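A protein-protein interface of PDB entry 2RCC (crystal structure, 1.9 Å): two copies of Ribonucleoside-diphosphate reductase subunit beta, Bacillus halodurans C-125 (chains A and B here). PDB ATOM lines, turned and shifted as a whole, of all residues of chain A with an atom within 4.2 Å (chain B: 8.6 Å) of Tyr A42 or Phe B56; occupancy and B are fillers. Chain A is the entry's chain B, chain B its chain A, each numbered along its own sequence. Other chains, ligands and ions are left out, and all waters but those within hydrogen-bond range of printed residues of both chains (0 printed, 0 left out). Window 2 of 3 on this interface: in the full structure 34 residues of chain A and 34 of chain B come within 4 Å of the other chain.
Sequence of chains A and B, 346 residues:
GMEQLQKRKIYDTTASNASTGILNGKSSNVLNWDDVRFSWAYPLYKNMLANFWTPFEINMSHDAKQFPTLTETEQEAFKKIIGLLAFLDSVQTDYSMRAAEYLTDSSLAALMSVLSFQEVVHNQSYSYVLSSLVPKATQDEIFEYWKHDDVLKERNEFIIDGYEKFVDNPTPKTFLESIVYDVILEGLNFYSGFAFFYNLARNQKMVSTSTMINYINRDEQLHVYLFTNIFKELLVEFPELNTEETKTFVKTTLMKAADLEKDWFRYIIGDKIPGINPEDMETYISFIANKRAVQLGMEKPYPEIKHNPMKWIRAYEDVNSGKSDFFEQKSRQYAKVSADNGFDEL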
ATOM      1  N   TRP A  40       5.355   2.060  27.461  1.00  0.00           N
ATOM      2  CA  TRP A  40       6.815   2.100  27.645  1.00  0.00           C
ATOM      3  C   TRP A  40       7.441   0.853  28.283  1.00  0.00           C
ATOM      4  O   TRP A  40       8.655   0.684  28.186  1.00  0.00           O
ATOM      5  CB  TRP A  40       7.232   3.332  28.469  1.00  0.00           C
ATOM      6  CG  TRP A  40       6.530   3.424  29.794  1.00  0.00           C
ATOM      7  CD1 TRP A  40       5.368   4.083  30.042  1.00  0.00           C
ATOM      8  CD2 TRP A  40       6.923   2.815  31.037  1.00  0.00           C
ATOM      9  NE1 TRP A  40       5.001   3.924  31.343  1.00  0.00           N
ATOM     10  CE2 TRP A  40       5.939   3.163  31.989  1.00  0.00           C
ATOM     11  CE3 TRP A  40       8.011   2.015  31.439  1.00  0.00           C
ATOM     12  CZ2 TRP A  40       5.996   2.732  33.322  1.00  0.00           C
ATOM     13  CZ3 TRP A  40       8.081   1.605  32.762  1.00  0.00           C
ATOM     14  CH2 TRP A  40       7.066   1.954  33.688  1.00  0.00           C
ATOM     15  N   ALA A  41       6.632  -0.014  28.898  1.00  0.00           N
ATOM     16  CA  ALA A  41       7.136  -1.202  29.611  1.00  0.00           C
ATOM     17  C   ALA A  41       7.877  -2.207  28.719  1.00  0.00           C
ATOM     18  O   ALA A  41       8.971  -2.585  29.040  1.00  0.00           O
ATOM     19  CB  ALA A  41       5.993  -1.904  30.347  1.00  0.00           C
ATOM     20  N   TYR A  42       7.292  -2.612  27.592  1.00  0.00           N
ATOM     21  CA  TYR A  42       7.964  -3.587  26.713  1.00  0.00           C
ATOM     22  C   TYR A  42       9.286  -3.072  26.110  1.00  0.00           C
ATOM     23  O   TYR A  42      10.281  -3.793  26.155  1.00  0.00           O
ATOM     24  CB  TYR A  42       7.011  -4.140  25.644  1.00  0.00           C
ATOM     25  CG  TYR A  42       7.556  -5.315  24.848  1.00  0.00           C
ATOM     26  CD1 TYR A  42       7.961  -6.496  25.486  1.00  0.00           C
ATOM     27  CD2 TYR A  42       7.595  -5.275  23.465  1.00  0.00           C
ATOM     28  CE1 TYR A  42       8.455  -7.569  24.771  1.00  0.00           C
ATOM     29  CE2 TYR A  42       8.073  -6.359  22.734  1.00  0.00           C
ATOM     30  CZ  TYR A  42       8.495  -7.498  23.395  1.00  0.00           C
ATOM     31  OH  TYR A  42       8.947  -8.561  22.664  1.00  0.00           O
ATOM     32  N   PRO A  43       9.313  -1.850  25.544  1.00  0.00           N
ATOM     33  CA  PRO A  43      10.609  -1.289  25.085  1.00  0.00           C
ATOM     34  C   PRO A  43      11.667  -1.193  26.183  1.00  0.00           C
ATOM     35  O   PRO A  43      12.857  -1.382  25.899  1.00  0.00           O
ATOM     36  CB  PRO A  43      10.240   0.122  24.619  1.00  0.00           C
ATOM     37  CG  PRO A  43       8.809   0.074  24.339  1.00  0.00           C
ATOM     38  CD  PRO A  43       8.185  -0.955  25.210  1.00  0.00           C
ATOM     39  N   LEU A  44      11.234  -0.905  27.412  1.00  0.00           N
ATOM     40  CA  LEU A  44      12.155  -0.872  28.562  1.00  0.00           C
ATOM     41  C   LEU A  44      12.696  -2.258  28.842  1.00  0.00           C
ATOM     42  O   LEU A  44      13.907  -2.412  29.017  1.00  0.00           O
ATOM     43  CB  LEU A  44      11.486  -0.281  29.821  1.00  0.00           C
ATOM     44  CG  LEU A  44      12.337  -0.154  31.081  1.00  0.00           C
ATOM     45  CD1 LEU A  44      13.560   0.705  30.773  1.00  0.00           C
ATOM     46  CD2 LEU A  44      11.513   0.385  32.237  1.00  0.00           C
ATOM     47  N   TYR A  45      11.806  -3.254  28.896  1.00  0.00           N
ATOM     48  CA  TYR A  45      12.195  -4.649  29.084  1.00  0.00           C
ATOM     49  C   TYR A  45      13.272  -5.063  28.055  1.00  0.00           C
ATOM     50  O   TYR A  45      14.323  -5.591  28.422  1.00  0.00           O
ATOM     51  CB  TYR A  45      10.963  -5.548  29.035  1.00  0.00           C
ATOM     52  CG  TYR A  45      11.254  -7.026  29.029  1.00  0.00           C
ATOM     53  CD1 TYR A  45      11.577  -7.696  30.210  1.00  0.00           C
ATOM     54  CD2 TYR A  45      11.170  -7.771  27.851  1.00  0.00           C
ATOM     55  CE1 TYR A  45      11.839  -9.036  30.207  1.00  0.00           C
ATOM     56  CE2 TYR A  45      11.435  -9.108  27.843  1.00  0.00           C
ATOM     57  CZ  TYR A  45      11.766  -9.754  29.027  1.00  0.00           C
ATOM     58  OH  TYR A  45      12.017 -11.109  29.035  1.00  0.00           O
ATOM     59  N   LYS A  46      13.004  -4.796  26.788  1.00  0.00           N
ATOM     60  CA  LYS A  46      13.952  -5.074  25.693  1.00  0.00           C
ATOM     61  C   LYS A  46      15.291  -4.355  25.843  1.00  0.00           C
ATOM     62  O   LYS A  46      16.354  -4.933  25.605  1.00  0.00           O
ATOM     63  CB  LYS A  46      13.334  -4.738  24.334  1.00  0.00           C
ATOM     64  CG  LYS A  46      12.261  -5.706  23.861  1.00  0.00           C
ATOM     65  CD  LYS A  46      11.881  -5.478  22.383  1.00  0.00           C
ATOM     66  CE  LYS A  46      11.182  -4.139  22.178  1.00  0.00           C
ATOM     67  N   LEU A  49      17.303  -6.007  28.789  1.00  0.00           N
ATOM     68  CA  LEU A  49      17.865  -7.264  28.314  1.00  0.00           C
ATOM     69  C   LEU A  49      19.026  -7.028  27.374  1.00  0.00           C
ATOM     70  O   LEU A  49      20.046  -7.710  27.485  1.00  0.00           O
ATOM     71  CB  LEU A  49      16.829  -8.125  27.606  1.00  0.00           C
ATOM     72  CG  LEU A  49      15.742  -8.829  28.427  1.00  0.00           C
ATOM     73  CD1 LEU A  49      14.954  -9.793  27.531  1.00  0.00           C
ATOM     74  CD2 LEU A  49      16.348  -9.612  29.592  1.00  0.00           C
ATOM     75  N   PHE B  52      23.560 -17.083  30.266  1.00  0.00           N
ATOM     76  CA  PHE B  52      22.593 -16.049  29.884  1.00  0.00           C
ATOM     77  C   PHE B  52      22.104 -16.266  28.446  1.00  0.00           C
ATOM     78  O   PHE B  52      22.901 -16.562  27.566  1.00  0.00           O
ATOM     79  CB  PHE B  52      23.201 -14.651  30.002  1.00  0.00           C
ATOM     80  CG  PHE B  52      22.223 -13.546  29.707  1.00  0.00           C
ATOM     81  CD1 PHE B  52      21.338 -13.121  30.685  1.00  0.00           C
ATOM     82  CD2 PHE B  52      22.166 -12.953  28.450  1.00  0.00           C
ATOM     83  CE1 PHE B  52      20.428 -12.089  30.414  1.00  0.00           C
ATOM     84  CE2 PHE B  52      21.248 -11.941  28.179  1.00  0.00           C
ATOM     85  CZ  PHE B  52      20.370 -11.527  29.164  1.00  0.00           C
ATOM     86  N   TRP B  53      20.796 -16.107  28.230  1.00  0.00           N
ATOM     87  CA  TRP B  53      20.200 -16.186  26.897  1.00  0.00           C
ATOM     88  C   TRP B  53      18.904 -15.384  26.914  1.00  0.00           C
ATOM     89  O   TRP B  53      18.346 -15.135  27.973  1.00  0.00           O
ATOM     90  CB  TRP B  53      19.914 -17.662  26.469  1.00  0.00           C
ATOM     91  CG  TRP B  53      18.884 -18.336  27.299  1.00  0.00           C
ATOM     92  CD1 TRP B  53      19.100 -18.974  28.479  1.00  0.00           C
ATOM     93  CD2 TRP B  53      17.460 -18.388  27.077  1.00  0.00           C
ATOM     94  NE1 TRP B  53      17.920 -19.412  29.002  1.00  0.00           N
ATOM     95  CE2 TRP B  53      16.898 -19.076  28.167  1.00  0.00           C
ATOM     96  CE3 TRP B  53      16.610 -17.932  26.060  1.00  0.00           C
ATOM     97  CZ2 TRP B  53      15.551 -19.337  28.262  1.00  0.00           C
ATOM     98  CZ3 TRP B  53      15.242 -18.207  26.164  1.00  0.00           C
ATOM     99  CH2 TRP B  53      14.737 -18.870  27.270  1.00  0.00           C
ATOM    100  N   THR B  54      18.451 -14.941  25.752  1.00  0.00           N
ATOM    101  CA  THR B  54      17.143 -14.313  25.654  1.00  0.00           C
ATOM    102  C   THR B  54      16.483 -14.859  24.403  1.00  0.00           C
ATOM    103  O   THR B  54      17.156 -15.294  23.481  1.00  0.00           O
ATOM    104  CB  THR B  54      17.140 -12.729  25.586  1.00  0.00           C
ATOM    105  OG1 THR B  54      17.446 -12.290  24.269  1.00  0.00           O
ATOM    106  CG2 THR B  54      18.074 -12.131  26.639  1.00  0.00           C
ATOM    107  N   PRO B  55      15.163 -14.833  24.357  1.00  0.00           N
ATOM    108  CA  PRO B  55      14.530 -15.337  23.120  1.00  0.00           C
ATOM    109  C   PRO B  55      14.812 -14.524  21.857  1.00  0.00           C
ATOM    110  O   PRO B  55      14.661 -15.040  20.771  1.00  0.00           O
ATOM    111  CB  PRO B  55      13.045 -15.321  23.473  1.00  0.00           C
ATOM    112  CG  PRO B  55      12.928 -14.317  24.547  1.00  0.00           C
ATOM    113  CD  PRO B  55      14.167 -14.417  25.356  1.00  0.00           C
ATOM    114  N   PHE B  56      15.296 -13.292  21.998  1.00  0.00           N
ATOM    115  CA  PHE B  56      15.568 -12.442  20.870  1.00  0.00           C
ATOM    116  C   PHE B  56      16.755 -12.879  20.020  1.00  0.00           C
ATOM    117  O   PHE B  56      16.902 -12.383  18.920  1.00  0.00           O
ATOM    118  CB  PHE B  56      15.717 -10.966  21.323  1.00  0.00           C
ATOM    119  CG  PHE B  56      14.492 -10.446  22.026  1.00  0.00           C
ATOM    120  CD1 PHE B  56      13.355 -10.125  21.313  1.00  0.00           C
ATOM    121  CD2 PHE B  56      14.451 -10.348  23.414  1.00  0.00           C
ATOM    122  CE1 PHE B  56      12.192  -9.669  21.961  1.00  0.00           C
ATOM    123  CE2 PHE B  56      13.302  -9.894  24.063  1.00  0.00           C
ATOM    124  CZ  PHE B  56      12.168  -9.549  23.324  1.00  0.00           C
ATOM    125  N   GLU B  57      17.584 -13.784  20.520  1.00  0.00           N
ATOM    126  CA  GLU B  57      18.694 -14.334  19.779  1.00  0.00           C
ATOM    127  C   GLU B  57      18.232 -15.531  18.897  1.00  0.00           C
ATOM    128  O   GLU B  57      19.009 -16.016  18.094  1.00  0.00           O
ATOM    129  CB  GLU B  57      19.811 -14.775  20.769  1.00  0.00           C
ATOM    130  CG  GLU B  57      19.617 -16.151  21.482  1.00  0.00           C
ATOM    131  CD  GLU B  57      20.546 -16.388  22.707  1.00  0.00           C
ATOM    132  OE1 GLU B  57      20.686 -15.498  23.605  1.00  0.00           O
ATOM    133  OE2 GLU B  57      21.113 -17.504  22.779  1.00  0.00           O
ATOM    134  N   ILE B  58      16.974 -15.975  19.039  1.00  0.00           N
ATOM    135  CA  ILE B  58      16.437 -17.142  18.315  1.00  0.00           C
ATOM    136  C   ILE B  58      15.458 -16.716  17.213  1.00  0.00           C
ATOM    137  O   ILE B  58      14.428 -16.087  17.479  1.00  0.00           O
ATOM    138  CB  ILE B  58      15.794 -18.105  19.313  1.00  0.00           C
ATOM    139  CG1 ILE B  58      16.909 -18.708  20.186  1.00  0.00           C
ATOM    140  CG2 ILE B  58      15.013 -19.206  18.580  1.00  0.00           C
ATOM    141  CD1 ILE B  58      16.420 -19.476  21.337  1.00  0.00           C
ATOM    142  N   ASN B  59      15.791 -17.058  15.970  1.00  0.00           N
ATOM    143  CA  ASN B  59      14.969 -16.682  14.834  1.00  0.00           C
ATOM    144  C   ASN B  59      13.905 -17.754  14.597  1.00  0.00           C
ATOM    145  O   ASN B  59      14.248 -18.913  14.380  1.00  0.00           O
ATOM    146  CB  ASN B  59      15.854 -16.514  13.600  1.00  0.00           C
ATOM    147  CG  ASN B  59      15.106 -15.909  12.405  1.00  0.00           C
ATOM    148  OD1 ASN B  59      14.005 -16.326  12.050  1.00  0.00           O
ATOM    149  ND2 ASN B  59      15.724 -14.927  11.776  1.00  0.00           N
ATOM    150  N   MET B  60      12.642 -17.347  14.560  1.00  0.00           N
ATOM    151  CA  MET B  60      11.511 -18.269  14.429  1.00  0.00           C
ATOM    152  C   MET B  60      10.943 -18.456  13.009  1.00  0.00           C
ATOM    153  O   MET B  60       9.932 -19.137  12.850  1.00  0.00           O
ATOM    154  CB  MET B  60      10.400 -17.811  15.387  1.00  0.00           C
ATOM    155  CG  MET B  60      10.707 -18.046  16.884  1.00  0.00           C
ATOM    156  SD  MET B  60      10.682 -19.871  17.328  1.00  0.00           S
ATOM    157  CE  MET B  60       8.909 -20.341  16.820  1.00  0.00           C
ATOM    158  N   VAL B 121      11.933 -14.239  32.002  1.00  0.00           N
ATOM    159  CA  VAL B 121      12.414 -14.503  30.662  1.00  0.00           C
ATOM    160  C   VAL B 121      11.811 -15.799  30.029  1.00  0.00           C
ATOM    161  O   VAL B 121      11.444 -15.793  28.833  1.00  0.00           O
ATOM    162  CB  VAL B 121      13.944 -14.522  30.571  1.00  0.00           C
ATOM    163  CG1 VAL B 121      14.368 -14.847  29.125  1.00  0.00           C
ATOM    164  CG2 VAL B 121      14.538 -13.144  31.009  1.00  0.00           C
ATOM    165  N   GLN B 124       8.205 -14.888  28.971  1.00  0.00           N
ATOM    166  CA  GLN B 124       8.234 -14.086  27.744  1.00  0.00           C
ATOM    167  C   GLN B 124       8.629 -14.915  26.485  1.00  0.00           C
ATOM    168  O   GLN B 124       8.171 -14.615  25.369  1.00  0.00           O
ATOM    169  CB  GLN B 124       9.128 -12.855  27.951  1.00  0.00           C
ATOM    170  CG  GLN B 124       9.258 -11.939  26.738  1.00  0.00           C
ATOM    171  CD  GLN B 124      10.571 -12.075  26.022  1.00  0.00           C
ATOM    172  OE1 GLN B 124      11.633 -12.256  26.646  1.00  0.00           O
ATOM    173  NE2 GLN B 124      10.536 -11.882  24.710  1.00  0.00           N
ATOM    174  N   SER B 125       9.496 -15.910  26.672  1.00  0.00           N
ATOM    175  CA  SER B 125       9.916 -16.800  25.604  1.00  0.00           C
ATOM    176  C   SER B 125       8.739 -17.651  25.116  1.00  0.00           C
ATOM    177  O   SER B 125       8.625 -17.937  23.933  1.00  0.00           O
ATOM    178  CB  SER B 125      11.079 -17.690  26.073  1.00  0.00           C
ATOM    179  OG  SER B 125      12.180 -16.916  26.515  1.00  0.00           O
ATOM    180  N   SER B 127       5.513 -16.745  25.165  1.00  0.00           N
ATOM    181  CA  SER B 127       4.751 -15.781  24.365  1.00  0.00           C
ATOM    182  C   SER B 127       5.374 -15.508  23.030  1.00  0.00           C
ATOM    183  O   SER B 127       4.679 -15.354  22.056  1.00  0.00           O
ATOM    184  CB  SER B 127       4.596 -14.436  25.089  1.00  0.00           C
ATOM    185  OG  SER B 127       3.818 -14.642  26.247  1.00  0.00           O
ATOM    186  N   TYR B 128       6.685 -15.360  23.018  1.00  0.00           N
ATOM    187  CA  TYR B 128       7.458 -15.117  21.796  1.00  0.00           C
ATOM    188  C   TYR B 128       7.276 -16.234  20.736  1.00  0.00           C
ATOM    189  O   TYR B 128       7.146 -15.954  19.532  1.00  0.00           O
ATOM    190  CB  TYR B 128       8.925 -14.954  22.210  1.00  0.00           C
ATOM    191  CG  TYR B 128       9.945 -14.685  21.139  1.00  0.00           C
ATOM    192  CD1 TYR B 128      10.375 -13.375  20.854  1.00  0.00           C
ATOM    193  CD2 TYR B 128      10.570 -15.736  20.483  1.00  0.00           C
ATOM    194  CE1 TYR B 128      11.358 -13.137  19.887  1.00  0.00           C
ATOM    195  CE2 TYR B 128      11.540 -15.513  19.504  1.00  0.00           C
ATOM    196  CZ  TYR B 128      11.939 -14.221  19.216  1.00  0.00           C
ATOM    197  OH  TYR B 128      12.938 -14.013  18.269  1.00  0.00           O
ATOM    198  N   SER B 131       3.453 -16.006  19.568  1.00  0.00           N
ATOM    199  CA  SER B 131       3.228 -14.840  18.726  1.00  0.00           C
ATOM    200  C   SER B 131       3.960 -14.905  17.379  1.00  0.00           C
ATOM    201  O   SER B 131       3.617 -14.171  16.469  1.00  0.00           O
ATOM    202  CB  SER B 131       3.595 -13.547  19.461  1.00  0.00           C
ATOM    203  OG  SER B 131       4.964 -13.530  19.771  1.00  0.00           O
ATOM    204  N   MET B 212      14.774 -23.266  22.481  1.00  0.00           N
ATOM    205  CA  MET B 212      14.396 -22.368  23.582  1.00  0.00           C
ATOM    206  C   MET B 212      13.881 -23.175  24.771  1.00  0.00           C
ATOM    207  O   MET B 212      14.218 -22.875  25.914  1.00  0.00           O
ATOM    208  CB  MET B 212      13.367 -21.340  23.115  1.00  0.00           C
ATOM    209  CG  MET B 212      13.661 -19.861  23.618  1.00  0.00           C
ATOM    210  SD  MET B 212      12.813 -18.800  22.358  1.00  0.00           S
ATOM    211  CE  MET B 212      11.085 -19.413  22.963  1.00  0.00           C
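OE1 of Gln B124 sits at hydrogen-bond distance from OH of Tyr A45 (2.7 Å).
OG1 of Thr B54 sits close to N of Phe B56 (3.3 Å).
The side-chain carboxylate of Glu B57 lies within hydrogen-bond range of the backbone NH of Thr B54.
The side-chain hydroxyl (OG) of Ser B125 lies within hydrogen-bond range of the backbone carbonyl oxygen (O) of Val B121 (2.7 Å).
Among the printed residues, pairs that only touch across the chains: Tyr A42 with Phe B56, Tyr A45 with Val B121, Lys A46 with Phe B56, Leu A49 with Thr B54 and Leu A49 with Phe B56.
Of chain B, only Phe B56 (3.4 Å) comes within 4 Å of Tyr A42.
Phe B56 touches just these residues of chain A: Tyr A42, Lys A46 and Leu A49.
No residue of chain B comes within 4 Å of Pro A43.
Printed residues of chain A within 4 Å of Thr B54: Leu A49.
Of the printed residues of chain B, Tyr A45 touches Val B121 and Gln B124.
Printed residues of chain B within 4 Å of Leu A49: Thr B54 and Phe B56.
Ile B58 touches none of the printed residues of chain A.
Leu A44 touches none of the printed residues of chain B.
The nearest printed residue of chain B that does not touch Lys A46 is Gln B124 (6.5 Å).
Of the 8 printed residues of chain A, 4 touch a printed residue of chain B.
Hydrophobic or aromatic side chains of chain A that line the printed part of chain B: Tyr A42, Tyr A45 and Leu A49.
Along chain A the printed residues that touch a printed residue of chain B span positions 42 to 49.
Printed residues of chain B that touch a printed residue of chain A: Thr B54, Phe B56, Val B121 and Gln B124.
Hydrophobic or aromatic side chains of chain B that line the printed part of chain A: Phe B56 and Val B121.
Among the printed residues, no Asp or Glu carboxylate lies within 4 Å of a Lys or Arg side-chain nitrogen of the other chain.
No position is printed for both chains.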
